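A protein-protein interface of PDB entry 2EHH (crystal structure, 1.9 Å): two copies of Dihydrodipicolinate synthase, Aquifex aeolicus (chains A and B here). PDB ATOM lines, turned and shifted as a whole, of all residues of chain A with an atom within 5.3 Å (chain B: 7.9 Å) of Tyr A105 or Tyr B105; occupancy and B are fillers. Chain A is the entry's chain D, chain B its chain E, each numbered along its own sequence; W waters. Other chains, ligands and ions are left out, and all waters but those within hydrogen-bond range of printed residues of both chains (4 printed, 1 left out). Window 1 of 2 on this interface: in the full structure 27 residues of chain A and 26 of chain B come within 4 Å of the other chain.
Tyr A105 touches its own counterpart, Tyr B105. Tyr A105 touches Tyr B106, and with the chains exchanged Tyr A106 touches Tyr B105. Asn A107 touches Arg B137, and with the chains exchanged Arg A137 touches Asn B107. Thr A138 touches Tyr B106, but with the chains exchanged Tyr A106 does not touch Thr B138 (4.04 Å). Positions printed for both chains: 77, 78, 79, 102, 103, 104, 105, 106, 107, 108, 137 and 138.
Of the 12 printed residues of chain A, 7 touch a printed residue of chain B. Printed residues of chain A that touch a printed residue of chain B: Asn A79, Val A102, Tyr A105, Tyr A106, Asn A107, Arg A137 and Thr A138. Among the printed residues, 17 pairs touch across the chains. Among the printed residues, no Asp or Glu carboxylate lies within 4 Å of a Lys or Arg side-chain nitrogen of the other chain.
The side-chain hydroxyl (OH) of Tyr A106 sits at hydrogen-bond distance from the side-chain hydroxyl (OG1) of Thr B43, at 2.6 Å. The guanidinium group of Arg B137 sits at hydrogen-bond distance from the backbone carbonyl oxygen of Tyr A106, 2.9 Å away. NH1 of Arg A137 lies within hydrogen-bond range of O of Tyr B106 (3.0 Å).
Among the printed residues, merely in contact across the chains: Asn A79 with Pro B48, Asn A79 with Pro B269, Val A102 with Tyr B106, Tyr A105 with Tyr B105, Tyr A105 with Tyr B106, Tyr A106 with Pro B48, Tyr A106 with Val B102, Tyr A106 with Tyr B105, Asn A107 with Pro B48, Asn A107 with Arg B137, Asn A107 with Pro B269, Arg A137 with Asn B107, Arg A137 with Cys B139 and Thr A138 with Tyr B106.
Tyr A105 touches just these residues of chain B: Tyr B105 (3.8 Å) and Tyr B106 (3.7 Å). Of the printed residues of chain B, Tyr A106 touches Thr B43 (2.6 Å), Pro B48 (3.7 Å), Val B102 (3.8 Å), Tyr B105 (3.7 Å) and Arg B137 (2.9 Å). Of the printed residues of chain B, Asn A107 touches Pro B48 (3.7 Å), Arg B137 (3.6 Å) and Pro B269 (3.6 Å). Of the printed residues of chain B, Arg A137 touches Tyr B106 (3.0 Å), Asn B107 (3.6 Å) and Cys B139 (3.6 Å). Val B103 touches none of the printed residues of chain A. Tyr B105 touches two residues of chain A. Pro B109 touches none of the printed residues of chain A. Of the printed residues of chain A, Arg B137 touches Tyr A106 and Asn A107. Printed residues of chain A within 4 Å of Pro B269: Asn A79 and Asn A107. The nearest residue of chain B that does not touch Tyr A105 is Asn B79 (4.7 Å).
The side-chain amide oxygen (OD1) of Asn A79 lies close to the backbone carbonyl oxygen (O) of Tyr A105 (3.0 Å). The backbone carbonyl oxygen (O) of Asn A79 sits at hydrogen-bond distance from the side-chain amide nitrogen (ND2) of Asn A107, at 2.9 Å. The backbone carbonyl oxygen of Tyr A105 lies close to the side-chain amide oxygen of Asn A107, at 3.3 Å. O of Thr A138 is in hydrogen-bond range of N of Tyr A106. The backbone carbonyl oxygen of Tyr B105 is in hydrogen-bond range of the side-chain amide nitrogen of Asn B79, 3.0 Å away. The backbone NH (N) of Tyr B106 lies within hydrogen-bond range of the backbone carbonyl oxygen (O) of Thr B138, 3.3 Å away.
Water W3 lies within hydrogen-bond range of the backbone carbonyl oxygen of Arg A137 (2.7 Å), the backbone carbonyl oxygen of Arg B137 (2.8 Å), the backbone NH of Tyr B106 (3.3 Å) and the backbone NH of Tyr A106 (3.3 Å). Water W4 lies within hydrogen-bond range of O of Asn A107 and NH1 of Arg B137. Water W1 bridges O of Asn B107 (2.8 Å) and NH1 of Arg A137 (3.1 Å). Water W2 bridges the side-chain hydroxyl (OH) of Tyr A105 (2.8 Å) and the side-chain amide nitrogen (ND2) of Asn B79 (3.0 Å).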
ATOM      1  N   GLY A  77     -27.661  -3.122 -11.449  1.00  0.00           N
ATOM      2  CA  GLY A  77     -27.237  -2.057 -12.341  1.00  0.00           C
ATOM      3  C   GLY A  77     -27.162  -2.389 -13.816  1.00  0.00           C
ATOM      4  O   GLY A  77     -27.201  -3.550 -14.212  1.00  0.00           O
ATOM      5  N   GLY A  78     -27.053  -1.340 -14.626  1.00  0.00           N
ATOM      6  CA  GLY A  78     -26.952  -1.473 -16.068  1.00  0.00           C
ATOM      7  C   GLY A  78     -26.333  -0.173 -16.548  1.00  0.00           C
ATOM      8  O   GLY A  78     -25.681   0.507 -15.760  1.00  0.00           O
ATOM      9  N   ASN A  79     -26.511   0.199 -17.811  1.00  0.00           N
ATOM     10  CA  ASN A  79     -25.927   1.462 -18.247  1.00  0.00           C
ATOM     11  C   ASN A  79     -26.987   2.539 -18.469  1.00  0.00           C
ATOM     12  O   ASN A  79     -26.755   3.525 -19.166  1.00  0.00           O
ATOM     13  CB  ASN A  79     -25.052   1.270 -19.498  1.00  0.00           C
ATOM     14  CG  ASN A  79     -25.816   0.710 -20.686  1.00  0.00           C
ATOM     15  OD1 ASN A  79     -25.233   0.453 -21.742  1.00  0.00           O
ATOM     16  ND2 ASN A  79     -27.115   0.525 -20.525  1.00  0.00           N
ATOM     17  N   VAL A 102     -23.133  -2.027 -11.038  1.00  0.00           N
ATOM     18  CA  VAL A 102     -21.962  -1.938 -11.901  1.00  0.00           C
ATOM     19  C   VAL A 102     -21.782  -0.549 -12.497  1.00  0.00           C
ATOM     20  O   VAL A 102     -22.747   0.191 -12.706  1.00  0.00           O
ATOM     21  CB  VAL A 102     -22.046  -2.971 -13.063  1.00  0.00           C
ATOM     22  CG1 VAL A 102     -23.126  -2.555 -14.051  1.00  0.00           C
ATOM     23  CG2 VAL A 102     -20.692  -3.107 -13.760  1.00  0.00           C
ATOM     24  N   VAL A 103     -20.530  -0.192 -12.747  1.00  0.00           N
ATOM     25  CA  VAL A 103     -20.222   1.077 -13.382  1.00  0.00           C
ATOM     26  C   VAL A 103     -20.798   0.895 -14.791  1.00  0.00           C
ATOM     27  O   VAL A 103     -20.577  -0.141 -15.417  1.00  0.00           O
ATOM     28  CB  VAL A 103     -18.693   1.279 -13.478  1.00  0.00           C
ATOM     29  CG1 VAL A 103     -18.373   2.486 -14.353  1.00  0.00           C
ATOM     30  CG2 VAL A 103     -18.105   1.457 -12.075  1.00  0.00           C
ATOM     31  N   PRO A 104     -21.560   1.880 -15.295  1.00  0.00           N
ATOM     32  CA  PRO A 104     -22.147   1.777 -16.637  1.00  0.00           C
ATOM     33  C   PRO A 104     -21.160   1.352 -17.722  1.00  0.00           C
ATOM     34  O   PRO A 104     -20.086   1.939 -17.879  1.00  0.00           O
ATOM     35  CB  PRO A 104     -22.702   3.175 -16.871  1.00  0.00           C
ATOM     36  CG  PRO A 104     -23.190   3.547 -15.499  1.00  0.00           C
ATOM     37  CD  PRO A 104     -22.024   3.104 -14.615  1.00  0.00           C
ATOM     38  N   TYR A 105     -21.546   0.329 -18.473  1.00  0.00           N
ATOM     39  CA  TYR A 105     -20.720  -0.200 -19.549  1.00  0.00           C
ATOM     40  C   TYR A 105     -21.169   0.320 -20.909  1.00  0.00           C
ATOM     41  O   TYR A 105     -22.305   0.772 -21.070  1.00  0.00           O
ATOM     42  CB  TYR A 105     -20.808  -1.728 -19.563  1.00  0.00           C
ATOM     43  CG  TYR A 105     -22.227  -2.237 -19.433  1.00  0.00           C
ATOM     44  CD1 TYR A 105     -22.715  -2.674 -18.204  1.00  0.00           C
ATOM     45  CD2 TYR A 105     -23.098  -2.241 -20.526  1.00  0.00           C
ATOM     46  CE1 TYR A 105     -24.030  -3.103 -18.061  1.00  0.00           C
ATOM     47  CE2 TYR A 105     -24.418  -2.667 -20.392  1.00  0.00           C
ATOM     48  CZ  TYR A 105     -24.874  -3.096 -19.154  1.00  0.00           C
ATOM     49  OH  TYR A 105     -26.173  -3.521 -19.007  1.00  0.00           O
ATOM     50  N   TYR A 106     -20.253   0.264 -21.869  1.00  0.00           N
ATOM     51  CA  TYR A 106     -20.510   0.653 -23.254  1.00  0.00           C
ATOM     52  C   TYR A 106     -20.694   2.139 -23.575  1.00  0.00           C
ATOM     53  O   TYR A 106     -20.078   2.628 -24.525  1.00  0.00           O
ATOM     54  CB  TYR A 106     -21.708  -0.146 -23.780  1.00  0.00           C
ATOM     55  CG  TYR A 106     -22.017   0.059 -25.250  1.00  0.00           C
ATOM     56  CD1 TYR A 106     -21.106  -0.316 -26.236  1.00  0.00           C
ATOM     57  CD2 TYR A 106     -23.235   0.606 -25.651  1.00  0.00           C
ATOM     58  CE1 TYR A 106     -21.407  -0.157 -27.596  1.00  0.00           C
ATOM     59  CE2 TYR A 106     -23.546   0.769 -26.997  1.00  0.00           C
ATOM     60  CZ  TYR A 106     -22.632   0.387 -27.964  1.00  0.00           C
ATOM     61  OH  TYR A 106     -22.959   0.544 -29.292  1.00  0.00           O
ATOM     62  N   ASN A 107     -21.524   2.862 -22.818  1.00  0.00           N
ATOM     63  CA  ASN A 107     -21.714   4.283 -23.131  1.00  0.00           C
ATOM     64  C   ASN A 107     -20.689   5.267 -22.554  1.00  0.00           C
ATOM     65  O   ASN A 107     -20.786   6.473 -22.775  1.00  0.00           O
ATOM     66  CB  ASN A 107     -23.163   4.749 -22.839  1.00  0.00           C
ATOM     67  CG  ASN A 107     -23.649   4.427 -21.432  1.00  0.00           C
ATOM     68  OD1 ASN A 107     -22.893   4.003 -20.566  1.00  0.00           O
ATOM     69  ND2 ASN A 107     -24.946   4.654 -21.201  1.00  0.00           N
ATOM     70  N   LYS A 108     -19.698   4.737 -21.839  1.00  0.00           N
ATOM     71  CA  LYS A 108     -18.594   5.519 -21.272  1.00  0.00           C
ATOM     72  C   LYS A 108     -18.921   6.907 -20.720  1.00  0.00           C
ATOM     73  O   LYS A 108     -18.403   7.921 -21.195  1.00  0.00           O
ATOM     74  CB  LYS A 108     -17.483   5.643 -22.322  1.00  0.00           C
ATOM     75  CG  LYS A 108     -16.973   4.290 -22.823  1.00  0.00           C
ATOM     76  CD  LYS A 108     -15.820   4.422 -23.822  1.00  0.00           C
ATOM     77  CE  LYS A 108     -14.595   5.050 -23.180  1.00  0.00           C
ATOM     78  NZ  LYS A 108     -13.410   5.011 -24.084  1.00  0.00           N
ATOM     79  N   ARG A 137     -14.484  -4.928 -18.742  1.00  0.00           N
ATOM     80  CA  ARG A 137     -15.795  -5.250 -19.307  1.00  0.00           C
ATOM     81  C   ARG A 137     -16.611  -3.994 -19.632  1.00  0.00           C
ATOM     82  O   ARG A 137     -17.263  -3.922 -20.673  1.00  0.00           O
ATOM     83  CB  ARG A 137     -16.616  -6.117 -18.336  1.00  0.00           C
ATOM     84  CG  ARG A 137     -16.166  -7.564 -18.212  1.00  0.00           C
ATOM     85  CD  ARG A 137     -17.022  -8.306 -17.189  1.00  0.00           C
ATOM     86  NE  ARG A 137     -16.634  -9.709 -17.073  1.00  0.00           N
ATOM     87  CZ  ARG A 137     -16.989 -10.665 -17.928  1.00  0.00           C
ATOM     88  NH1 ARG A 137     -17.755 -10.380 -18.971  1.00  0.00           N
ATOM     89  NH2 ARG A 137     -16.565 -11.909 -17.742  1.00  0.00           N
ATOM     90  N   THR A 138     -16.573  -3.009 -18.743  1.00  0.00           N
ATOM     91  CA  THR A 138     -17.352  -1.784 -18.932  1.00  0.00           C
ATOM     92  C   THR A 138     -16.679  -0.787 -19.862  1.00  0.00           C
ATOM     93  O   THR A 138     -17.332   0.114 -20.394  1.00  0.00           O
ATOM     94  CB  THR A 138     -17.600  -1.076 -17.598  1.00  0.00           C
ATOM     95  OG1 THR A 138     -16.354  -0.594 -17.094  1.00  0.00           O
ATOM     96  CG2 THR A 138     -18.218  -2.039 -16.582  1.00  0.00           C
ATOM     97  N   THR B  43     -25.115   4.091 -31.203  1.00  0.00           N
ATOM     98  CA  THR B  43     -24.515   4.602 -29.978  1.00  0.00           C
ATOM     99  C   THR B  43     -24.726   6.112 -29.897  1.00  0.00           C
ATOM    100  O   THR B  43     -25.042   6.661 -28.833  1.00  0.00           O
ATOM    101  CB  THR B  43     -23.002   4.332 -29.954  1.00  0.00           C
ATOM    102  OG1 THR B  43     -22.768   2.946 -30.218  1.00  0.00           O
ATOM    103  CG2 THR B  43     -22.422   4.700 -28.597  1.00  0.00           C
ATOM    104  N   SER B  47     -28.857   4.637 -27.802  1.00  0.00           N
ATOM    105  CA  SER B  47     -29.596   3.383 -27.698  1.00  0.00           C
ATOM    106  C   SER B  47     -29.562   2.785 -26.281  1.00  0.00           C
ATOM    107  O   SER B  47     -30.543   2.195 -25.828  1.00  0.00           O
ATOM    108  CB  SER B  47     -29.055   2.364 -28.705  1.00  0.00           C
ATOM    109  OG  SER B  47     -27.657   2.194 -28.556  1.00  0.00           O
ATOM    110  N   PRO B  48     -28.435   2.932 -25.564  1.00  0.00           N
ATOM    111  CA  PRO B  48     -28.361   2.377 -24.206  1.00  0.00           C
ATOM    112  C   PRO B  48     -29.471   2.822 -23.254  1.00  0.00           C
ATOM    113  O   PRO B  48     -29.932   2.036 -22.424  1.00  0.00           O
ATOM    114  CB  PRO B  48     -26.991   2.834 -23.727  1.00  0.00           C
ATOM    115  CG  PRO B  48     -26.181   2.792 -24.983  1.00  0.00           C
ATOM    116  CD  PRO B  48     -27.119   3.447 -25.984  1.00  0.00           C
ATOM    117  N   HIS B  55     -37.122   2.116 -29.084  1.00  0.00           N
ATOM    118  CA  HIS B  55     -36.313   1.693 -30.227  1.00  0.00           C
ATOM    119  C   HIS B  55     -37.265   1.409 -31.382  1.00  0.00           C
ATOM    120  O   HIS B  55     -37.099   1.922 -32.487  1.00  0.00           O
ATOM    121  CB  HIS B  55     -35.546   0.398 -29.930  1.00  0.00           C
ATOM    122  CG  HIS B  55     -34.159   0.606 -29.403  1.00  0.00           C
ATOM    123  ND1 HIS B  55     -33.898   0.894 -28.081  1.00  0.00           N
ATOM    124  CD2 HIS B  55     -32.954   0.517 -30.014  1.00  0.00           C
ATOM    125  CE1 HIS B  55     -32.592   0.968 -27.899  1.00  0.00           C
ATOM    126  NE2 HIS B  55     -31.995   0.743 -29.056  1.00  0.00           N
ATOM    127  N   GLY B  77     -28.949  -4.003 -32.291  1.00  0.00           N
ATOM    128  CA  GLY B  77     -28.223  -4.939 -31.451  1.00  0.00           C
ATOM    129  C   GLY B  77     -28.122  -4.614 -29.973  1.00  0.00           C
ATOM    130  O   GLY B  77     -28.549  -3.556 -29.513  1.00  0.00           O
ATOM    131  N   GLY B  78     -27.546  -5.556 -29.238  1.00  0.00           N
ATOM    132  CA  GLY B  78     -27.343  -5.424 -27.805  1.00  0.00           C
ATOM    133  C   GLY B  78     -26.447  -6.589 -27.438  1.00  0.00           C
ATOM    134  O   GLY B  78     -25.795  -7.142 -28.322  1.00  0.00           O
ATOM    135  N   ASN B  79     -26.395  -6.982 -26.168  1.00  0.00           N
ATOM    136  CA  ASN B  79     -25.543  -8.110 -25.820  1.00  0.00           C
ATOM    137  C   ASN B  79     -26.322  -9.387 -25.486  1.00  0.00           C
ATOM    138  O   ASN B  79     -25.788 -10.310 -24.875  1.00  0.00           O
ATOM    139  CB  ASN B  79     -24.572  -7.741 -24.685  1.00  0.00           C
ATOM    140  CG  ASN B  79     -25.272  -7.365 -23.395  1.00  0.00           C
ATOM    141  OD1 ASN B  79     -26.492  -7.437 -23.283  1.00  0.00           O
ATOM    142  ND2 ASN B  79     -24.487  -6.962 -22.403  1.00  0.00           N
ATOM    143  N   ALA B  80     -27.586  -9.424 -25.900  1.00  0.00           N
ATOM    144  CA  ALA B  80     -28.450 -10.591 -25.700  1.00  0.00           C
ATOM    145  C   ALA B  80     -28.978 -10.964 -27.082  1.00  0.00           C
ATOM    146  O   ALA B  80     -29.673 -10.180 -27.731  1.00  0.00           O
ATOM    147  CB  ALA B  80     -29.603 -10.255 -24.765  1.00  0.00           C
ATOM    148  N   GLU B  83     -33.090 -10.857 -27.864  1.00  0.00           N
ATOM    149  CA  GLU B  83     -33.671  -9.545 -28.120  1.00  0.00           C
ATOM    150  C   GLU B  83     -33.152  -8.904 -29.396  1.00  0.00           C
ATOM    151  O   GLU B  83     -33.871  -8.134 -30.028  1.00  0.00           O
ATOM    152  CB  GLU B  83     -33.473  -8.592 -26.931  1.00  0.00           C
ATOM    153  CG  GLU B  83     -32.106  -8.589 -26.291  1.00  0.00           C
ATOM    154  CD  GLU B  83     -31.983  -7.514 -25.212  1.00  0.00           C
ATOM    155  OE1 GLU B  83     -31.106  -7.649 -24.329  1.00  0.00           O
ATOM    156  OE2 GLU B  83     -32.759  -6.528 -25.251  1.00  0.00           O
ATOM    157  N   VAL B 102     -24.466  -4.266 -33.318  1.00  0.00           N
ATOM    158  CA  VAL B 102     -23.192  -4.100 -32.633  1.00  0.00           C
ATOM    159  C   VAL B 102     -22.652  -5.411 -32.070  1.00  0.00           C
ATOM    160  O   VAL B 102     -23.413  -6.327 -31.752  1.00  0.00           O
ATOM    161  CB  VAL B 102     -23.319  -3.079 -31.466  1.00  0.00           C
ATOM    162  CG1 VAL B 102     -24.226  -3.638 -30.377  1.00  0.00           C
ATOM    163  CG2 VAL B 102     -21.950  -2.752 -30.903  1.00  0.00           C
ATOM    164  N   VAL B 103     -21.331  -5.503 -31.977  1.00  0.00           N
ATOM    165  CA  VAL B 103     -20.678  -6.669 -31.395  1.00  0.00           C
ATOM    166  C   VAL B 103     -21.072  -6.598 -29.915  1.00  0.00           C
ATOM    167  O   VAL B 103     -20.888  -5.563 -29.280  1.00  0.00           O
ATOM    168  CB  VAL B 103     -19.136  -6.549 -31.506  1.00  0.00           C
ATOM    169  CG1 VAL B 103     -18.463  -7.612 -30.653  1.00  0.00           C
ATOM    170  CG2 VAL B 103     -18.701  -6.682 -32.967  1.00  0.00           C
ATOM    171  N   PRO B 104     -21.638  -7.680 -29.356  1.00  0.00           N
ATOM    172  CA  PRO B 104     -22.047  -7.694 -27.946  1.00  0.00           C
ATOM    173  C   PRO B 104     -21.036  -7.065 -26.989  1.00  0.00           C
ATOM    174  O   PRO B 104     -19.868  -7.455 -26.954  1.00  0.00           O
ATOM    175  CB  PRO B 104     -22.265  -9.175 -27.675  1.00  0.00           C
ATOM    176  CG  PRO B 104     -22.878  -9.630 -28.969  1.00  0.00           C
ATOM    177  CD  PRO B 104     -21.990  -8.957 -30.010  1.00  0.00           C
ATOM    178  N   TYR B 105     -21.503  -6.086 -26.219  1.00  0.00           N
ATOM    179  CA  TYR B 105     -20.669  -5.382 -25.254  1.00  0.00           C
ATOM    180  C   TYR B 105     -20.793  -5.996 -23.860  1.00  0.00           C
ATOM    181  O   TYR B 105     -21.759  -6.697 -23.559  1.00  0.00           O
ATOM    182  CB  TYR B 105     -21.092  -3.906 -25.179  1.00  0.00           C
ATOM    183  CG  TYR B 105     -22.599  -3.716 -25.162  1.00  0.00           C
ATOM    184  CD1 TYR B 105     -23.294  -3.406 -26.328  1.00  0.00           C
ATOM    185  CD2 TYR B 105     -23.331  -3.908 -23.993  1.00  0.00           C
ATOM    186  CE1 TYR B 105     -24.682  -3.294 -26.333  1.00  0.00           C
ATOM    187  CE2 TYR B 105     -24.721  -3.800 -23.985  1.00  0.00           C
ATOM    188  CZ  TYR B 105     -25.387  -3.492 -25.159  1.00  0.00           C
ATOM    189  OH  TYR B 105     -26.758  -3.376 -25.161  1.00  0.00           O
ATOM    190  N   TYR B 106     -19.796  -5.732 -23.025  1.00  0.00           N
ATOM    191  CA  TYR B 106     -19.791  -6.172 -21.636  1.00  0.00           C
ATOM    192  C   TYR B 106     -19.659  -7.658 -21.291  1.00  0.00           C
ATOM    193  O   TYR B 106     -18.856  -8.000 -20.418  1.00  0.00           O
ATOM    194  CB  TYR B 106     -21.024  -5.605 -20.929  1.00  0.00           C
ATOM    195  CG  TYR B 106     -21.029  -5.858 -19.438  1.00  0.00           C
ATOM    196  CD1 TYR B 106     -20.091  -5.251 -18.605  1.00  0.00           C
ATOM    197  CD2 TYR B 106     -21.953  -6.724 -18.867  1.00  0.00           C
ATOM    198  CE1 TYR B 106     -20.074  -5.504 -17.231  1.00  0.00           C
ATOM    199  CE2 TYR B 106     -21.950  -6.983 -17.497  1.00  0.00           C
ATOM    200  CZ  TYR B 106     -21.009  -6.371 -16.688  1.00  0.00           C
ATOM    201  OH  TYR B 106     -21.014  -6.626 -15.335  1.00  0.00           O
ATOM    202  N   ASN B 107     -20.428  -8.544 -21.928  1.00  0.00           N
ATOM    203  CA  ASN B 107     -20.298  -9.958 -21.573  1.00  0.00           C
ATOM    204  C   ASN B 107     -19.180 -10.705 -22.297  1.00  0.00           C
ATOM    205  O   ASN B 107     -18.965 -11.890 -22.062  1.00  0.00           O
ATOM    206  CB  ASN B 107     -21.639 -10.720 -21.692  1.00  0.00           C
ATOM    207  CG  ASN B 107     -22.355 -10.505 -23.016  1.00  0.00           C
ATOM    208  OD1 ASN B 107     -21.811  -9.940 -23.964  1.00  0.00           O
ATOM    209  ND2 ASN B 107     -23.598 -10.979 -23.083  1.00  0.00           N
ATOM    210  N   LYS B 108     -18.462  -9.995 -23.166  1.00  0.00           N
ATOM    211  CA  LYS B 108     -17.319 -10.541 -23.891  1.00  0.00           C
ATOM    212  C   LYS B 108     -17.432 -11.979 -24.391  1.00  0.00           C
ATOM    213  O   LYS B 108     -16.676 -12.862 -23.965  1.00  0.00           O
ATOM    214  CB  LYS B 108     -16.069 -10.416 -23.016  1.00  0.00           C
ATOM    215  CG  LYS B 108     -15.755  -8.979 -22.607  1.00  0.00           C
ATOM    216  CD  LYS B 108     -14.497  -8.877 -21.751  1.00  0.00           C
ATOM    217  CE  LYS B 108     -13.267  -9.350 -22.513  1.00  0.00           C
ATOM    218  NZ  LYS B 108     -12.005  -9.084 -21.755  1.00  0.00           N
ATOM    219  N   PRO B 109     -18.362 -12.239 -25.312  1.00  0.00           N
ATOM    220  CA  PRO B 109     -18.458 -13.622 -25.790  1.00  0.00           C
ATOM    221  C   PRO B 109     -17.206 -14.096 -26.523  1.00  0.00           C
ATOM    222  O   PRO B 109     -16.389 -13.291 -26.977  1.00  0.00           O
ATOM    223  CB  PRO B 109     -19.692 -13.602 -26.697  1.00  0.00           C
ATOM    224  CG  PRO B 109     -19.853 -12.164 -27.078  1.00  0.00           C
ATOM    225  CD  PRO B 109     -19.442 -11.397 -25.855  1.00  0.00           C
ATOM    226  N   LEU B 114     -19.663 -15.047 -30.839  1.00  0.00           N
ATOM    227  CA  LEU B 114     -19.932 -13.942 -31.752  1.00  0.00           C
ATOM    228  C   LEU B 114     -20.461 -14.500 -33.069  1.00  0.00           C
ATOM    229  O   LEU B 114     -21.347 -13.918 -33.694  1.00  0.00           O
ATOM    230  CB  LEU B 114     -18.655 -13.128 -31.996  1.00  0.00           C
ATOM    231  CG  LEU B 114     -18.069 -12.439 -30.759  1.00  0.00           C
ATOM    232  CD1 LEU B 114     -16.804 -11.684 -31.146  1.00  0.00           C
ATOM    233  CD2 LEU B 114     -19.100 -11.479 -30.172  1.00  0.00           C
ATOM    234  N   HIS B 117     -24.022 -15.552 -32.456  1.00  0.00           N
ATOM    235  CA  HIS B 117     -24.857 -14.372 -32.238  1.00  0.00           C
ATOM    236  C   HIS B 117     -25.300 -13.797 -33.588  1.00  0.00           C
ATOM    237  O   HIS B 117     -26.496 -13.703 -33.873  1.00  0.00           O
ATOM    238  CB  HIS B 117     -24.066 -13.314 -31.460  1.00  0.00           C
ATOM    239  CG  HIS B 117     -24.799 -12.024 -31.263  1.00  0.00           C
ATOM    240  ND1 HIS B 117     -25.848 -11.887 -30.378  1.00  0.00           N
ATOM    241  CD2 HIS B 117     -24.618 -10.802 -31.821  1.00  0.00           C
ATOM    242  CE1 HIS B 117     -26.279 -10.640 -30.396  1.00  0.00           C
ATOM    243  NE2 HIS B 117     -25.549  -9.958 -31.263  1.00  0.00           N
ATOM    244  N   ILE B 134     -16.569  -1.984 -32.395  1.00  0.00           N
ATOM    245  CA  ILE B 134     -16.011  -0.838 -31.683  1.00  0.00           C
ATOM    246  C   ILE B 134     -15.485  -1.336 -30.345  1.00  0.00           C
ATOM    247  O   ILE B 134     -16.136  -1.196 -29.313  1.00  0.00           O
ATOM    248  CB  ILE B 134     -17.065   0.275 -31.473  1.00  0.00           C
ATOM    249  CG1 ILE B 134     -16.452   1.425 -30.669  1.00  0.00           C
ATOM    250  CG2 ILE B 134     -18.312  -0.286 -30.796  1.00  0.00           C
ATOM    251  CD1 ILE B 134     -17.234   2.726 -30.785  1.00  0.00           C
ATOM    252  N   ARG B 137     -15.544   0.391 -26.855  1.00  0.00           N
ATOM    253  CA  ARG B 137     -16.791   0.459 -26.095  1.00  0.00           C
ATOM    254  C   ARG B 137     -17.310  -0.907 -25.658  1.00  0.00           C
ATOM    255  O   ARG B 137     -17.782  -1.068 -24.528  1.00  0.00           O
ATOM    256  CB  ARG B 137     -17.880   1.150 -26.914  1.00  0.00           C
ATOM    257  CG  ARG B 137     -17.694   2.650 -27.096  1.00  0.00           C
ATOM    258  CD  ARG B 137     -18.866   3.215 -27.883  1.00  0.00           C
ATOM    259  NE  ARG B 137     -18.783   4.663 -28.049  1.00  0.00           N
ATOM    260  CZ  ARG B 137     -19.159   5.550 -27.132  1.00  0.00           C
ATOM    261  NH1 ARG B 137     -19.655   5.141 -25.971  1.00  0.00           N
ATOM    262  NH2 ARG B 137     -19.029   6.848 -27.376  1.00  0.00           N
ATOM    263  N   THR B 138     -17.224  -1.887 -26.551  1.00  0.00           N
ATOM    264  CA  THR B 138     -17.718  -3.232 -26.267  1.00  0.00           C
ATOM    265  C   THR B 138     -16.740  -4.045 -25.440  1.00  0.00           C
ATOM    266  O   THR B 138     -17.126  -5.001 -24.768  1.00  0.00           O
ATOM    267  CB  THR B 138     -17.998  -4.008 -27.566  1.00  0.00           C
ATOM    268  OG1 THR B 138     -16.762  -4.250 -28.247  1.00  0.00           O
ATOM    269  CG2 THR B 138     -18.922  -3.214 -28.471  1.00  0.00           C
ATOM    270  N   CYS B 139     -15.473  -3.662 -25.504  1.00  0.00           N
ATOM    271  CA  CYS B 139     -14.421  -4.334 -24.762  1.00  0.00           C
ATOM    272  C   CYS B 139     -14.120  -5.760 -25.265  1.00  0.00           C
ATOM    273  O   CYS B 139     -13.610  -6.615 -24.533  1.00  0.00           O
ATOM    274  CB  CYS B 139     -14.763  -4.282 -23.259  1.00  0.00           C
ATOM    275  SG  CYS B 139     -13.747  -3.047 -22.360  1.00  0.00           S
ATOM    276  N   VAL B 140     -14.430  -5.999 -26.537  1.00  0.00           N
ATOM    277  CA  VAL B 140     -14.164  -7.275 -27.198  1.00  0.00           C
ATOM    278  C   VAL B 140     -14.131  -6.957 -28.694  1.00  0.00           C
ATOM    279  O   VAL B 140     -14.658  -5.932 -29.115  1.00  0.00           O
ATOM    280  CB  VAL B 140     -15.262  -8.335 -26.899  1.00  0.00           C
ATOM    281  CG1 VAL B 140     -16.540  -8.023 -27.672  1.00  0.00           C
ATOM    282  CG2 VAL B 140     -14.747  -9.733 -27.243  1.00  0.00           C
ATOM    283  N   PRO B 269     -26.935   7.694 -17.600  1.00  0.00           N
ATOM    284  CA  PRO B 269     -25.713   8.355 -17.140  1.00  0.00           C
ATOM    285  C   PRO B 269     -25.063   9.433 -18.006  1.00  0.00           C
ATOM    286  O   PRO B 269     -24.041   9.984 -17.609  1.00  0.00           O
ATOM    287  CB  PRO B 269     -24.774   7.179 -16.894  1.00  0.00           C
ATOM    288  CG  PRO B 269     -25.120   6.274 -18.007  1.00  0.00           C
ATOM    289  CD  PRO B 269     -26.642   6.306 -18.003  1.00  0.00           C
HETATM  290  O   HOH W   1     -19.726 -12.703 -19.503  1.00  0.00           O
HETATM  291  O   HOH W   2     -26.004  -6.121 -20.016  1.00  0.00           O
HETATM  292  O   HOH W   3     -18.843  -2.658 -22.494  1.00  0.00           O
HETATM  293  O   HOH W   4     -21.959   7.012 -25.215  1.00  0.00           O
